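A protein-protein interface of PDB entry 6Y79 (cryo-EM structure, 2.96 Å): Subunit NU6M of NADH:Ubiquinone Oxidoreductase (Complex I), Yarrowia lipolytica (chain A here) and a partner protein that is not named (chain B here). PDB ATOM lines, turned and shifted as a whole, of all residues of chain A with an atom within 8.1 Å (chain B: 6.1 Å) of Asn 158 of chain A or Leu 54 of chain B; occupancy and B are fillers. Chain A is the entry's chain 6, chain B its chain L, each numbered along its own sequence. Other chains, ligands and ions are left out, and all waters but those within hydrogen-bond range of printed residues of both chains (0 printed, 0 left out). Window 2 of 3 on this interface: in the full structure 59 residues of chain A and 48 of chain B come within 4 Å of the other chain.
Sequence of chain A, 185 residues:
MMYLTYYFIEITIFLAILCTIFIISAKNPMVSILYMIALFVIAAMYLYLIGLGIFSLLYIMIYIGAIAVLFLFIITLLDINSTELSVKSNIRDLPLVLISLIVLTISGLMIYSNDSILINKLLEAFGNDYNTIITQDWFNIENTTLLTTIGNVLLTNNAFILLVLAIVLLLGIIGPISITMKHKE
OG of Ser 44 of chain B is in hydrogen-bond range of OG of Ser 53 of chain B (3.1 Å). O of Val 153 of chain A sits at hydrogen-bond distance from N of Asn 158 of chain A (2.8 Å).
Among the printed residues, merely in contact across the chains: Phe 55 of chain A with Ser 53 of chain B (3.6 Å), Thr 149 of chain A with Ile 50 of chain B (3.7 Å), Ile 150 of chain A with Ile 57 of chain B (3.7 Å), Val 153 of chain A with Ile 50 of chain B (3.6 Å), Val 153 of chain A with Leu 54 of chain B (3.7 Å) and Asn 158 of chain A with Leu 54 of chain B (3.3 Å).
Of the printed residues of chain B, Phe 55 of chain A touches Ser 53. Of the printed residues of chain B, Val 153 of chain A touches Ile 50 (3.6 Å) and Leu 54 (3.7 Å). Asn 157 of chain A touches none of the printed residues of chain B. Asn 158 of chain A touches just one residue of chain B: Leu 54 (3.3 Å). Of the printed residues of chain A, Ile 50 of chain B touches Thr 149 and Val 153. Of the printed residues of chain A, Ser 53 of chain B touches Phe 55 (3.6 Å).
Of the 18 printed residues of chain A, 5 touch a printed residue of chain B. Hydrophobic or aromatic side chains of chain A within 4 Å of the printed part of chain B: Phe 55, Ile 150 and Val 153. Of the 11 printed residues of chain B, 4 touch a printed residue of chain A. Hydrophobic or aromatic side chains of chain B that line the printed part of chain A: Ile 50, Leu 54 and Ile 57. Among the printed residues, 6 pairs touch across the chains. Among the printed residues, no Asp or Glu carboxylate lies within 4 Å of a Lys or Arg side-chain nitrogen of the other chain.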
ATOM      1  N   PHE A  55      -7.580  13.223  31.699  1.00  0.00           N
ATOM      2  CA  PHE A  55      -7.177  13.950  32.896  1.00  0.00           C
ATOM      3  C   PHE A  55      -7.327  13.112  34.142  1.00  0.00           C
ATOM      4  O   PHE A  55      -6.519  13.240  35.056  1.00  0.00           O
ATOM      5  CB  PHE A  55      -7.988  15.223  33.062  1.00  0.00           C
ATOM      6  CG  PHE A  55      -7.571  16.320  32.162  1.00  0.00           C
ATOM      7  CD1 PHE A  55      -6.376  16.987  32.358  1.00  0.00           C
ATOM      8  CD2 PHE A  55      -8.380  16.696  31.121  1.00  0.00           C
ATOM      9  CE1 PHE A  55      -6.003  18.003  31.517  1.00  0.00           C
ATOM     10  CE2 PHE A  55      -8.028  17.714  30.296  1.00  0.00           C
ATOM     11  CZ  PHE A  55      -6.828  18.362  30.481  1.00  0.00           C
ATOM     12  N   LEU A 146      -6.899  14.978  22.939  1.00  0.00           N
ATOM     13  CA  LEU A 146      -6.616  16.158  23.743  1.00  0.00           C
ATOM     14  C   LEU A 146      -5.151  16.223  24.160  1.00  0.00           C
ATOM     15  O   LEU A 146      -4.571  17.314  24.246  1.00  0.00           O
ATOM     16  CB  LEU A 146      -7.549  16.150  24.947  1.00  0.00           C
ATOM     17  CG  LEU A 146      -7.523  17.258  25.974  1.00  0.00           C
ATOM     18  CD1 LEU A 146      -8.931  17.574  26.349  1.00  0.00           C
ATOM     19  CD2 LEU A 146      -6.795  16.737  27.162  1.00  0.00           C
ATOM     20  N   THR A 149      -3.069  17.756  21.351  1.00  0.00           N
ATOM     21  CA  THR A 149      -3.105  19.203  21.200  1.00  0.00           C
ATOM     22  C   THR A 149      -2.408  19.894  22.365  1.00  0.00           C
ATOM     23  O   THR A 149      -1.811  20.962  22.175  1.00  0.00           O
ATOM     24  CB  THR A 149      -4.545  19.682  21.057  1.00  0.00           C
ATOM     25  OG1 THR A 149      -5.225  18.815  20.150  1.00  0.00           O
ATOM     26  CG2 THR A 149      -4.563  21.104  20.496  1.00  0.00           C
ATOM     27  N   ILE A 150      -2.435  19.290  23.560  1.00  0.00           N
ATOM     28  CA  ILE A 150      -1.615  19.801  24.658  1.00  0.00           C
ATOM     29  C   ILE A 150      -0.136  19.704  24.302  1.00  0.00           C
ATOM     30  O   ILE A 150       0.638  20.638  24.537  1.00  0.00           O
ATOM     31  CB  ILE A 150      -1.937  19.069  25.975  1.00  0.00           C
ATOM     32  CG1 ILE A 150      -3.330  19.446  26.460  1.00  0.00           C
ATOM     33  CG2 ILE A 150      -0.962  19.451  27.062  1.00  0.00           C
ATOM     34  CD1 ILE A 150      -3.733  18.755  27.734  1.00  0.00           C
ATOM     35  N   ASN A 152       0.957  19.872  21.242  1.00  0.00           N
ATOM     36  CA  ASN A 152       1.272  20.817  20.177  1.00  0.00           C
ATOM     37  C   ASN A 152       1.442  22.218  20.719  1.00  0.00           C
ATOM     38  O   ASN A 152       2.329  22.945  20.275  1.00  0.00           O
ATOM     39  CB  ASN A 152       0.174  20.819  19.105  1.00  0.00           C
ATOM     40  CG  ASN A 152       0.578  21.530  17.809  1.00  0.00           C
ATOM     41  OD1 ASN A 152       1.709  21.991  17.648  1.00  0.00           O
ATOM     42  ND2 ASN A 152      -0.376  21.660  16.890  1.00  0.00           N
ATOM     43  N   VAL A 153       0.658  22.594  21.719  1.00  0.00           N
ATOM     44  CA  VAL A 153       0.654  23.986  22.135  1.00  0.00           C
ATOM     45  C   VAL A 153       1.578  24.250  23.326  1.00  0.00           C
ATOM     46  O   VAL A 153       2.095  25.359  23.467  1.00  0.00           O
ATOM     47  CB  VAL A 153      -0.801  24.395  22.379  1.00  0.00           C
ATOM     48  CG1 VAL A 153      -0.916  25.854  22.592  1.00  0.00           C
ATOM     49  CG2 VAL A 153      -1.555  24.082  21.130  1.00  0.00           C
ATOM     50  N   LEU A 154       1.898  23.235  24.134  1.00  0.00           N
ATOM     51  CA  LEU A 154       3.046  23.353  25.030  1.00  0.00           C
ATOM     52  C   LEU A 154       4.362  23.479  24.282  1.00  0.00           C
ATOM     53  O   LEU A 154       5.342  23.954  24.856  1.00  0.00           O
ATOM     54  CB  LEU A 154       3.167  22.142  25.947  1.00  0.00           C
ATOM     55  CG  LEU A 154       2.351  21.980  27.216  1.00  0.00           C
ATOM     56  CD1 LEU A 154       2.608  20.591  27.762  1.00  0.00           C
ATOM     57  CD2 LEU A 154       2.748  23.034  28.218  1.00  0.00           C
ATOM     58  N   LEU A 155       4.413  23.054  23.023  1.00  0.00           N
ATOM     59  CA  LEU A 155       5.670  22.886  22.319  1.00  0.00           C
ATOM     60  C   LEU A 155       5.892  23.868  21.187  1.00  0.00           C
ATOM     61  O   LEU A 155       7.024  23.983  20.712  1.00  0.00           O
ATOM     62  CB  LEU A 155       5.776  21.467  21.750  1.00  0.00           C
ATOM     63  CG  LEU A 155       6.340  20.369  22.650  1.00  0.00           C
ATOM     64  CD1 LEU A 155       7.660  20.876  23.075  1.00  0.00           C
ATOM     65  CD2 LEU A 155       5.516  19.984  23.867  1.00  0.00           C
ATOM     66  N   THR A 156       4.851  24.543  20.718  1.00  0.00           N
ATOM     67  CA  THR A 156       4.996  25.550  19.678  1.00  0.00           C
ATOM     68  C   THR A 156       4.600  26.935  20.159  1.00  0.00           C
ATOM     69  O   THR A 156       5.420  27.854  20.123  1.00  0.00           O
ATOM     70  CB  THR A 156       4.152  25.156  18.470  1.00  0.00           C
ATOM     71  OG1 THR A 156       2.869  24.696  18.908  1.00  0.00           O
ATOM     72  CG2 THR A 156       4.835  24.091  17.697  1.00  0.00           C
ATOM     73  N   ASN A 157       3.369  27.099  20.625  1.00  0.00           N
ATOM     74  CA  ASN A 157       2.863  28.416  20.963  1.00  0.00           C
ATOM     75  C   ASN A 157       3.260  28.828  22.366  1.00  0.00           C
ATOM     76  O   ASN A 157       3.421  30.021  22.637  1.00  0.00           O
ATOM     77  CB  ASN A 157       1.349  28.422  20.828  1.00  0.00           C
ATOM     78  CG  ASN A 157       0.901  28.249  19.412  1.00  0.00           C
ATOM     79  OD1 ASN A 157       1.247  29.040  18.544  1.00  0.00           O
ATOM     80  ND2 ASN A 157       0.132  27.207  19.160  1.00  0.00           N
ATOM     81  N   ASN A 158       3.423  27.865  23.259  1.00  0.00           N
ATOM     82  CA  ASN A 158       3.780  28.123  24.639  1.00  0.00           C
ATOM     83  C   ASN A 158       5.018  27.338  25.004  1.00  0.00           C
ATOM     84  O   ASN A 158       5.087  26.698  26.053  1.00  0.00           O
ATOM     85  CB  ASN A 158       2.612  27.799  25.557  1.00  0.00           C
ATOM     86  CG  ASN A 158       1.390  28.599  25.214  1.00  0.00           C
ATOM     87  OD1 ASN A 158       0.426  28.075  24.689  1.00  0.00           O
ATOM     88  ND2 ASN A 158       1.432  29.885  25.495  1.00  0.00           N
ATOM     89  N   ALA A 159       6.010  27.370  24.114  1.00  0.00           N
ATOM     90  CA  ALA A 159       7.276  26.693  24.358  1.00  0.00           C
ATOM     91  C   ALA A 159       8.052  27.369  25.475  1.00  0.00           C
ATOM     92  O   ALA A 159       8.739  26.705  26.264  1.00  0.00           O
ATOM     93  CB  ALA A 159       8.096  26.673  23.073  1.00  0.00           C
ATOM     94  N   PHE A 160       7.941  28.694  25.560  1.00  0.00           N
ATOM     95  CA  PHE A 160       8.591  29.448  26.619  1.00  0.00           C
ATOM     96  C   PHE A 160       8.014  29.104  27.984  1.00  0.00           C
ATOM     97  O   PHE A 160       8.753  29.089  28.973  1.00  0.00           O
ATOM     98  CB  PHE A 160       8.458  30.939  26.322  1.00  0.00           C
ATOM     99  CG  PHE A 160       9.109  31.823  27.333  1.00  0.00           C
ATOM    100  CD1 PHE A 160      10.474  32.029  27.308  1.00  0.00           C
ATOM    101  CD2 PHE A 160       8.355  32.460  28.299  1.00  0.00           C
ATOM    102  CE1 PHE A 160      11.070  32.838  28.231  1.00  0.00           C
ATOM    103  CE2 PHE A 160       8.950  33.264  29.224  1.00  0.00           C
ATOM    104  CZ  PHE A 160      10.309  33.455  29.189  1.00  0.00           C
ATOM    105  N   ILE A 161       6.714  28.808  28.054  1.00  0.00           N
ATOM    106  CA  ILE A 161       6.101  28.391  29.313  1.00  0.00           C
ATOM    107  C   ILE A 161       6.641  27.039  29.742  1.00  0.00           C
ATOM    108  O   ILE A 161       6.911  26.813  30.923  1.00  0.00           O
ATOM    109  CB  ILE A 161       4.570  28.382  29.176  1.00  0.00           C
ATOM    110  CG1 ILE A 161       4.068  29.799  28.970  1.00  0.00           C
ATOM    111  CG2 ILE A 161       3.893  27.803  30.401  1.00  0.00           C
ATOM    112  CD1 ILE A 161       2.629  29.861  28.682  1.00  0.00           C
ATOM    113  N   LEU A 162       6.880  26.151  28.777  1.00  0.00           N
ATOM    114  CA  LEU A 162       7.487  24.857  29.065  1.00  0.00           C
ATOM    115  C   LEU A 162       8.926  24.996  29.543  1.00  0.00           C
ATOM    116  O   LEU A 162       9.350  24.268  30.445  1.00  0.00           O
ATOM    117  CB  LEU A 162       7.381  23.977  27.819  1.00  0.00           C
ATOM    118  CG  LEU A 162       7.803  22.514  27.756  1.00  0.00           C
ATOM    119  CD1 LEU A 162       6.775  21.760  26.966  1.00  0.00           C
ATOM    120  CD2 LEU A 162       9.138  22.397  27.051  1.00  0.00           C
ATOM    121  N   LEU A 163       9.672  25.970  29.025  1.00  0.00           N
ATOM    122  CA  LEU A 163      11.058  26.115  29.470  1.00  0.00           C
ATOM    123  C   LEU A 163      11.174  26.832  30.821  1.00  0.00           C
ATOM    124  O   LEU A 163      12.033  26.488  31.648  1.00  0.00           O
ATOM    125  CB  LEU A 163      11.867  26.828  28.393  1.00  0.00           C
ATOM    126  CG  LEU A 163      11.984  26.125  27.034  1.00  0.00           C
ATOM    127  CD1 LEU A 163      13.143  26.679  26.271  1.00  0.00           C
ATOM    128  CD2 LEU A 163      12.156  24.633  27.174  1.00  0.00           C
ATOM    129  N   VAL A 164      10.308  27.812  31.087  1.00  0.00           N
ATOM    130  CA  VAL A 164      10.238  28.396  32.427  1.00  0.00           C
ATOM    131  C   VAL A 164       9.736  27.361  33.427  1.00  0.00           C
ATOM    132  O   VAL A 164      10.176  27.323  34.585  1.00  0.00           O
ATOM    133  CB  VAL A 164       9.366  29.669  32.385  1.00  0.00           C
ATOM    134  CG1 VAL A 164       9.166  30.257  33.754  1.00  0.00           C
ATOM    135  CG2 VAL A 164      10.032  30.692  31.522  1.00  0.00           C
ATOM    136  N   LEU A 165       8.883  26.447  32.970  1.00  0.00           N
ATOM    137  CA  LEU A 165       8.443  25.330  33.791  1.00  0.00           C
ATOM    138  C   LEU A 165       9.586  24.367  34.084  1.00  0.00           C
ATOM    139  O   LEU A 165       9.631  23.756  35.156  1.00  0.00           O
ATOM    140  CB  LEU A 165       7.306  24.626  33.066  1.00  0.00           C
ATOM    141  CG  LEU A 165       6.392  23.673  33.793  1.00  0.00           C
ATOM    142  CD1 LEU A 165       5.638  24.428  34.856  1.00  0.00           C
ATOM    143  CD2 LEU A 165       5.450  23.103  32.767  1.00  0.00           C
ATOM    144  N   SER B  44     -13.146  24.698  30.094  1.00  0.00           N
ATOM    145  CA  SER B  44     -12.482  24.302  28.857  1.00  0.00           C
ATOM    146  C   SER B  44     -13.363  23.384  28.024  1.00  0.00           C
ATOM    147  O   SER B  44     -13.398  23.488  26.792  1.00  0.00           O
ATOM    148  CB  SER B  44     -11.162  23.612  29.182  1.00  0.00           C
ATOM    149  OG  SER B  44     -10.516  23.163  28.010  1.00  0.00           O
ATOM    150  N   ILE B  50      -8.604  24.165  24.332  1.00  0.00           N
ATOM    151  CA  ILE B  50      -7.521  23.556  25.097  1.00  0.00           C
ATOM    152  C   ILE B  50      -6.833  24.491  26.063  1.00  0.00           C
ATOM    153  O   ILE B  50      -5.860  24.078  26.707  1.00  0.00           O
ATOM    154  CB  ILE B  50      -6.325  23.125  24.241  1.00  0.00           C
ATOM    155  CG1 ILE B  50      -6.008  24.297  23.330  1.00  0.00           C
ATOM    156  CG2 ILE B  50      -6.602  21.862  23.498  1.00  0.00           C
ATOM    157  CD1 ILE B  50      -4.628  24.361  22.992  1.00  0.00           C
ATOM    158  N   SER B  51      -7.227  25.758  26.119  1.00  0.00           N
ATOM    159  CA  SER B  51      -6.348  26.733  26.745  1.00  0.00           C
ATOM    160  C   SER B  51      -6.540  26.711  28.245  1.00  0.00           C
ATOM    161  O   SER B  51      -5.588  26.919  29.014  1.00  0.00           O
ATOM    162  CB  SER B  51      -6.611  28.115  26.164  1.00  0.00           C
ATOM    163  OG  SER B  51      -5.420  28.828  26.171  1.00  0.00           O
ATOM    164  N   GLY B  52      -7.776  26.458  28.669  1.00  0.00           N
ATOM    165  CA  GLY B  52      -8.012  26.038  30.031  1.00  0.00           C
ATOM    166  C   GLY B  52      -7.365  24.708  30.355  1.00  0.00           C
ATOM    167  O   GLY B  52      -6.857  24.524  31.460  1.00  0.00           O
ATOM    168  N   SER B  53      -7.310  23.786  29.386  1.00  0.00           N
ATOM    169  CA  SER B  53      -6.583  22.538  29.600  1.00  0.00           C
ATOM    170  C   SER B  53      -5.082  22.790  29.695  1.00  0.00           C
ATOM    171  O   SER B  53      -4.383  22.085  30.425  1.00  0.00           O
ATOM    172  CB  SER B  53      -6.894  21.551  28.477  1.00  0.00           C
ATOM    173  OG  SER B  53      -8.235  21.103  28.532  1.00  0.00           O
ATOM    174  N   LEU B  54      -4.585  23.808  28.994  1.00  0.00           N
ATOM    175  CA  LEU B  54      -3.180  24.193  29.080  1.00  0.00           C
ATOM    176  C   LEU B  54      -2.839  24.738  30.461  1.00  0.00           C
ATOM    177  O   LEU B  54      -1.856  24.311  31.081  1.00  0.00           O
ATOM    178  CB  LEU B  54      -2.889  25.229  27.999  1.00  0.00           C
ATOM    179  CG  LEU B  54      -1.515  25.679  27.531  1.00  0.00           C
ATOM    180  CD1 LEU B  54      -1.749  26.114  26.141  1.00  0.00           C
ATOM    181  CD2 LEU B  54      -1.019  26.854  28.301  1.00  0.00           C
ATOM    182  N   PHE B  55      -3.648  25.683  30.962  1.00  0.00           N
ATOM    183  CA  PHE B  55      -3.415  26.212  32.303  1.00  0.00           C
ATOM    184  C   PHE B  55      -3.604  25.140  33.366  1.00  0.00           C
ATOM    185  O   PHE B  55      -2.908  25.155  34.384  1.00  0.00           O
ATOM    186  CB  PHE B  55      -4.327  27.412  32.570  1.00  0.00           C
ATOM    187  CG  PHE B  55      -4.029  28.151  33.859  1.00  0.00           C
ATOM    188  CD1 PHE B  55      -3.026  29.093  33.929  1.00  0.00           C
ATOM    189  CD2 PHE B  55      -4.781  27.919  34.994  1.00  0.00           C
ATOM    190  CE1 PHE B  55      -2.773  29.768  35.106  1.00  0.00           C
ATOM    191  CE2 PHE B  55      -4.536  28.590  36.171  1.00  0.00           C
ATOM    192  CZ  PHE B  55      -3.532  29.514  36.226  1.00  0.00           C
ATOM    193  N   ALA B  56      -4.478  24.161  33.115  1.00  0.00           N
ATOM    194  CA  ALA B  56      -4.696  23.087  34.079  1.00  0.00           C
ATOM    195  C   ALA B  56      -3.522  22.116  34.122  1.00  0.00           C
ATOM    196  O   ALA B  56      -3.103  21.688  35.204  1.00  0.00           O
ATOM    197  CB  ALA B  56      -5.991  22.350  33.756  1.00  0.00           C
ATOM    198  N   ILE B  57      -2.963  21.758  32.961  1.00  0.00           N
ATOM    199  CA  ILE B  57      -1.799  20.878  32.981  1.00  0.00           C
ATOM    200  C   ILE B  57      -0.568  21.598  33.526  1.00  0.00           C
ATOM    201  O   ILE B  57       0.319  20.953  34.090  1.00  0.00           O
ATOM    202  CB  ILE B  57      -1.539  20.249  31.592  1.00  0.00           C
ATOM    203  CG1 ILE B  57      -0.700  18.981  31.744  1.00  0.00           C
ATOM    204  CG2 ILE B  57      -0.843  21.203  30.639  1.00  0.00           C
ATOM    205  CD1 ILE B  57      -0.532  18.189  30.496  1.00  0.00           C
ATOM    206  N   VAL B  58      -0.510  22.926  33.435  1.00  0.00           N
ATOM    207  CA  VAL B  58       0.620  23.627  34.034  1.00  0.00           C
ATOM    208  C   VAL B  58       0.455  23.741  35.550  1.00  0.00           C
ATOM    209  O   VAL B  58       1.413  23.555  36.316  1.00  0.00           O
ATOM    210  CB  VAL B  58       0.783  24.991  33.344  1.00  0.00           C
ATOM    211  CG1 VAL B  58       1.727  25.857  34.092  1.00  0.00           C
ATOM    212  CG2 VAL B  58       1.304  24.785  31.937  1.00  0.00           C
ATOM    213  N   ILE B  59      -0.768  23.986  36.017  1.00  0.00           N
ATOM    214  CA  ILE B  59      -0.991  24.117  37.449  1.00  0.00           C
ATOM    215  C   ILE B  59      -0.950  22.769  38.177  1.00  0.00           C
ATOM    216  O   ILE B  59      -0.696  22.749  39.386  1.00  0.00           O
ATOM    217  CB  ILE B  59      -2.304  24.891  37.669  1.00  0.00           C
ATOM    218  CG1 ILE B  59      -2.404  25.476  39.070  1.00  0.00           C
ATOM    219  CG2 ILE B  59      -3.462  24.031  37.455  1.00  0.00           C
ATOM    220  CD1 ILE B  59      -3.623  26.336  39.257  1.00  0.00           C
